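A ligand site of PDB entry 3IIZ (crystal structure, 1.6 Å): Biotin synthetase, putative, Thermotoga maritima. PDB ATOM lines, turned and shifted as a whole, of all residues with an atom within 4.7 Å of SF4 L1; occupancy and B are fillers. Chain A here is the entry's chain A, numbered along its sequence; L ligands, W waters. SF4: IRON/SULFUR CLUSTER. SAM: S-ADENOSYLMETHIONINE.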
ATOM      1  N   CYS A  63      -5.072  33.755  12.769  1.00  0.00           N
ATOM      2  CA  CYS A  63      -3.896  32.927  12.630  1.00  0.00           C
ATOM      3  C   CYS A  63      -3.811  32.224  11.284  1.00  0.00           C
ATOM      4  O   CYS A  63      -4.809  31.741  10.752  1.00  0.00           O
ATOM      5  CB  CYS A  63      -3.836  31.884  13.738  1.00  0.00           C
ATOM      6  SG  CYS A  63      -2.208  31.152  13.838  1.00  0.00           S
ATOM      7  N   LYS A  65      -1.731  29.572  10.884  1.00  0.00           N
ATOM      8  CA  LYS A  65      -1.323  28.197  11.135  1.00  0.00           C
ATOM      9  C   LYS A  65      -2.542  27.368  11.566  1.00  0.00           C
ATOM     10  O   LYS A  65      -3.602  27.923  11.826  1.00  0.00           O
ATOM     11  CB  LYS A  65      -0.230  28.163  12.196  1.00  0.00           C
ATOM     12  CG  LYS A  65       1.176  28.440  11.638  1.00  0.00           C
ATOM     13  CD  LYS A  65       2.238  28.187  12.672  1.00  0.00           C
ATOM     14  CE  LYS A  65       3.640  28.111  12.078  1.00  0.00           C
ATOM     15  NZ  LYS A  65       4.064  29.293  11.266  1.00  0.00           N
ATOM     16  N   ASN A  66      -2.383  26.054  11.607  1.00  0.00           N
ATOM     17  CA  ASN A  66      -3.491  25.152  11.758  1.00  0.00           C
ATOM     18  C   ASN A  66      -3.239  24.134  12.860  1.00  0.00           C
ATOM     19  O   ASN A  66      -3.679  22.987  12.748  1.00  0.00           O
ATOM     20  CB  ASN A  66      -3.774  24.463  10.421  1.00  0.00           C
ATOM     21  CG  ASN A  66      -5.222  24.110  10.226  1.00  0.00           C
ATOM     22  OD1 ASN A  66      -6.117  24.702  10.793  1.00  0.00           O
ATOM     23  ND2 ASN A  66      -5.460  23.128   9.327  1.00  0.00           N
ATOM     24  N   CYS A  67      -2.540  24.545  13.914  1.00  0.00           N
ATOM     25  CA  CYS A  67      -2.197  23.628  15.005  1.00  0.00           C
ATOM     26  C   CYS A  67      -3.427  22.869  15.455  1.00  0.00           C
ATOM     27  O   CYS A  67      -4.509  23.461  15.644  1.00  0.00           O
ATOM     28  CB  CYS A  67      -1.597  24.380  16.192  1.00  0.00           C
ATOM     29  SG  CYS A  67      -0.156  25.422  15.741  1.00  0.00           S
ATOM     30  N   TYR A  69      -4.459  21.423  18.158  1.00  0.00           N
ATOM     31  CA  TYR A  69      -4.969  21.644  19.508  1.00  0.00           C
ATOM     32  C   TYR A  69      -5.671  22.972  19.729  1.00  0.00           C
ATOM     33  O   TYR A  69      -6.418  23.145  20.719  1.00  0.00           O
ATOM     34  CB  TYR A  69      -3.835  21.561  20.532  1.00  0.00           C
ATOM     35  CG  TYR A  69      -2.579  22.262  20.143  1.00  0.00           C
ATOM     36  CD1 TYR A  69      -2.417  23.646  20.362  1.00  0.00           C
ATOM     37  CD2 TYR A  69      -1.517  21.546  19.610  1.00  0.00           C
ATOM     38  CE1 TYR A  69      -1.216  24.302  20.017  1.00  0.00           C
ATOM     39  CE2 TYR A  69      -0.305  22.196  19.270  1.00  0.00           C
ATOM     40  CZ  TYR A  69      -0.184  23.560  19.467  1.00  0.00           C
ATOM     41  OH  TYR A  69       0.981  24.156  19.135  1.00  0.00           O
ATOM     42  N   CYS A  70      -5.437  23.924  18.835  1.00  0.00           N
ATOM     43  CA  CYS A  70      -5.717  25.326  19.121  1.00  0.00           C
ATOM     44  C   CYS A  70      -7.023  25.804  18.503  1.00  0.00           C
ATOM     45  O   CYS A  70      -7.239  25.622  17.288  1.00  0.00           O
ATOM     46  CB  CYS A  70      -4.595  26.188  18.577  1.00  0.00           C
ATOM     47  SG  CYS A  70      -4.764  27.920  19.051  1.00  0.00           S
ATOM     48  N   LEU A  72      -7.814  28.788  17.748  1.00  0.00           N
ATOM     49  CA  LEU A  72      -7.594  29.838  16.760  1.00  0.00           C
ATOM     50  C   LEU A  72      -7.062  29.312  15.400  1.00  0.00           C
ATOM     51  O   LEU A  72      -6.828  30.120  14.489  1.00  0.00           O
ATOM     52  CB  LEU A  72      -6.604  30.909  17.273  1.00  0.00           C
ATOM     53  CG  LEU A  72      -6.853  31.436  18.663  1.00  0.00           C
ATOM     54  CD1 LEU A  72      -5.967  32.628  18.900  1.00  0.00           C
ATOM     55  CD2 LEU A  72      -8.302  31.835  18.851  1.00  0.00           C
ATOM     56  N   ARG A  73      -6.889  28.003  15.278  1.00  0.00           N
ATOM     57  CA  ARG A  73      -6.373  27.399  14.036  1.00  0.00           C
ATOM     58  C   ARG A  73      -7.158  27.889  12.841  1.00  0.00           C
ATOM     59  O   ARG A  73      -8.350  28.134  12.921  1.00  0.00           O
ATOM     60  CB  ARG A  73      -6.446  25.879  14.091  1.00  0.00           C
ATOM     61  CG  ARG A  73      -7.840  25.274  14.212  1.00  0.00           C
ATOM     62  CD  ARG A  73      -7.758  23.812  14.688  1.00  0.00           C
ATOM     63  NE  ARG A  73      -6.799  22.991  13.915  1.00  0.00           N
ATOM     64  CZ  ARG A  73      -7.101  22.295  12.812  1.00  0.00           C
ATOM     65  NH1 ARG A  73      -8.338  22.304  12.305  1.00  0.00           N
ATOM     66  NH2 ARG A  73      -6.175  21.602  12.197  1.00  0.00           N
ATOM     67  N   SER A 108      -0.708  37.051  20.161  1.00  0.00           N
ATOM     68  CA  SER A 108      -1.661  36.935  19.094  1.00  0.00           C
ATOM     69  C   SER A 108      -1.587  35.600  18.430  1.00  0.00           C
ATOM     70  O   SER A 108      -0.615  34.859  18.592  1.00  0.00           O
ATOM     71  CB  SER A 108      -1.431  38.032  18.051  1.00  0.00           C
ATOM     72  OG  SER A 108      -0.134  37.953  17.453  1.00  0.00           O
ATOM     73  N   GLY A 109      -2.583  35.332  17.593  1.00  0.00           N
ATOM     74  CA  GLY A 109      -2.401  34.344  16.535  1.00  0.00           C
ATOM     75  C   GLY A 109      -1.268  34.820  15.628  1.00  0.00           C
ATOM     76  O   GLY A 109      -0.845  35.983  15.690  1.00  0.00           O
ATOM     77  N   GLU A 110      -0.776  33.933  14.765  1.00  0.00           N
ATOM     78  CA  GLU A 110       0.168  34.352  13.722  1.00  0.00           C
ATOM     79  C   GLU A 110      -0.579  35.081  12.637  1.00  0.00           C
ATOM     80  O   GLU A 110      -0.940  34.507  11.638  1.00  0.00           O
ATOM     81  CB  GLU A 110       0.951  33.172  13.155  1.00  0.00           C
ATOM     82  CG  GLU A 110       1.909  32.544  14.171  1.00  0.00           C
ATOM     83  CD  GLU A 110       2.931  31.603  13.527  1.00  0.00           C
ATOM     84  OE1 GLU A 110       2.976  31.557  12.281  1.00  0.00           O
ATOM     85  OE2 GLU A 110       3.683  30.937  14.278  1.00  0.00           O
ATOM     86  N   ARG A 172       1.430  20.240  14.654  1.00  0.00           N
ATOM     87  CA  ARG A 172       1.697  21.574  14.102  1.00  0.00           C
ATOM     88  C   ARG A 172       2.136  21.375  12.660  1.00  0.00           C
ATOM     89  O   ARG A 172       3.331  21.519  12.332  1.00  0.00           O
ATOM     90  CB  ARG A 172       2.755  22.260  14.928  1.00  0.00           C
ATOM     91  CG  ARG A 172       2.419  22.204  16.450  1.00  0.00           C
ATOM     92  CD  ARG A 172       3.329  23.043  17.331  1.00  0.00           C
ATOM     93  NE  ARG A 172       3.054  24.442  17.034  1.00  0.00           N
ATOM     94  CZ  ARG A 172       3.874  25.270  16.417  1.00  0.00           C
ATOM     95  NH1 ARG A 172       5.124  24.918  16.153  1.00  0.00           N
ATOM     96  NH2 ARG A 172       3.454  26.483  16.123  1.00  0.00           N
HETATM   97 FE1  SF4 L   1      -0.909  27.509  16.501  1.00  0.00          FE
HETATM   98 FE2  SF4 L   1      -0.391  29.842  18.014  1.00  0.00          FE
HETATM   99 FE3  SF4 L   1      -2.026  29.837  15.690  1.00  0.00          FE
HETATM  100 FE4  SF4 L   1      -2.952  28.644  17.887  1.00  0.00          FE
HETATM  101  S1  SF4 L   1      -2.508  30.832  17.708  1.00  0.00           S
HETATM  102  S2  SF4 L   1      -3.042  27.845  15.709  1.00  0.00           S
HETATM  103  S3  SF4 L   1      -1.021  27.799  18.813  1.00  0.00           S
HETATM  104  S4  SF4 L   1       0.240  29.341  15.832  1.00  0.00           S
HETATM  105  N   SAM L   2       0.545  31.976  18.106  1.00  0.00           N
HETATM  106  CA  SAM L   2       1.578  32.120  19.164  1.00  0.00           C
HETATM  107  C   SAM L   2       2.191  30.729  19.396  1.00  0.00           C
HETATM  108  O   SAM L   2       1.641  29.713  18.965  1.00  0.00           O
HETATM  109  OXT SAM L   2       3.240  30.590  20.032  1.00  0.00           O
HETATM  110  CB  SAM L   2       0.991  32.728  20.440  1.00  0.00           C
HETATM  111  CG  SAM L   2      -0.444  32.340  20.779  1.00  0.00           C
HETATM  112  SD  SAM L   2      -0.714  30.588  21.157  1.00  0.00           S
HETATM  113  CE  SAM L   2      -2.487  30.551  21.464  1.00  0.00           C
HETATM  114  C5' SAM L   2      -0.105  30.473  22.876  1.00  0.00           C
HETATM  115  C4' SAM L   2       0.034  29.109  23.558  1.00  0.00           C
HETATM  116  O4' SAM L   2      -1.264  28.595  23.823  1.00  0.00           O
HETATM  117  C3' SAM L   2       0.713  28.011  22.775  1.00  0.00           C
HETATM  118  O3' SAM L   2       2.113  28.085  22.903  1.00  0.00           O
HETATM  119  C2' SAM L   2       0.120  26.734  23.378  1.00  0.00           C
HETATM  120  O2' SAM L   2       0.962  26.045  24.278  1.00  0.00           O
HETATM  121  C1' SAM L   2      -1.142  27.226  24.135  1.00  0.00           C
HETATM  122  N9  SAM L   2      -2.315  26.511  23.680  1.00  0.00           N
HETATM  123  C8  SAM L   2      -2.910  26.553  22.445  1.00  0.00           C
HETATM  124  N7  SAM L   2      -3.970  25.702  22.443  1.00  0.00           N
HETATM  125  C5  SAM L   2      -4.045  25.094  23.656  1.00  0.00           C
HETATM  126  C6  SAM L   2      -4.910  24.143  24.197  1.00  0.00           C
HETATM  127  N6  SAM L   2      -5.915  23.598  23.496  1.00  0.00           N
HETATM  128  N1  SAM L   2      -4.740  23.780  25.520  1.00  0.00           N
HETATM  129  C2  SAM L   2      -3.733  24.293  26.268  1.00  0.00           C
HETATM  130  N3  SAM L   2      -2.884  25.228  25.725  1.00  0.00           N
HETATM  131  C4  SAM L   2      -3.026  25.604  24.443  1.00  0.00           C
HETATM  132  O   HOH W   1       3.367  29.651  16.547  1.00  0.00           O
HETATM  133  O   HOH W   2       2.005  26.709  18.980  1.00  0.00           O
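An iron atom (FE2) of SF4 L1 is bound by an oxygen (O) of SAM L2, 2.2 Å away.
Water W2 lies within hydrogen-bond range of the side-chain hydroxyl of Tyr 69 (2.8 Å), the guanidinium group of Arg 172 (3.2 Å) and a sulfur (S3) of SF4 L1 (3.2 Å).
Water W1 lies within hydrogen-bond range of OE2 of Glu 110, NH2 of Arg 172 and S4 of SF4 L1.
The side-chain sulfur (SG) of Cys 70 sits close to the backbone NH (N) of Leu 72, at 3.4 Å.
The backbone NH of Lys 65 sits close to the side-chain sulfur of Cys 63 (3.4 Å).
The side-chain sulfur (SG) of Cys 67 sits close to the side-chain hydroxyl (OH) of Tyr 69 (3.8 Å).
The guanidinium group (NE) of Arg 73 sits at hydrogen-bond distance from the backbone carbonyl oxygen (O) of Cys 67, 2.9 Å away.
The side-chain sulfur (SG) of Cys 67 lies close to the guanidinium group (NE) of Arg 172, 3.6 Å away.
The side-chain hydroxyl (OH) of Tyr 69 sits at hydrogen-bond distance from the guanidinium group (NE) of Arg 172 (3.0 Å).
O of Asn 66 is in hydrogen-bond range of NH2 of Arg 73 (2.9 Å).
NZ of Lys 65 is in salt-bridge range of OE1 of Glu 110, 2.7 Å away.
FE4 of SF4 L1 is bound by SG of Cys 70 (2.3 Å).
FE3 of SF4 L1 is bound by SG of Cys 63 (2.3 Å).
The backbone NH of Cys 67 sits close to a sulfur (S2) of SF4 L1 (3.8 Å).
FE1 of SF4 L1 is bound by SG of Cys 67 (2.3 Å).
A nitrogen (N6) of SAM L2 is in hydrogen-bond range of the backbone carbonyl oxygen of Tyr 69 (2.9 Å).
O of Ser 108 sits close to N of SAM L2 (3.1 Å).
Residues that only touch SF4 L1: Lys 65 (3.9 Å), Tyr 69 (3.7 Å), Arg 73 (3.8 Å), Gly 109 (3.7 Å) and Glu 110 (3.98 Å).
Hydrophobic or aromatic side chains that line SF4 L1: Tyr 69.
Eight residues have an atom within 4 Å of SF4 L1: Cys 63, Lys 65, Cys 67, Tyr 69, Cys 70, Arg 73, Gly 109 and Glu 110.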
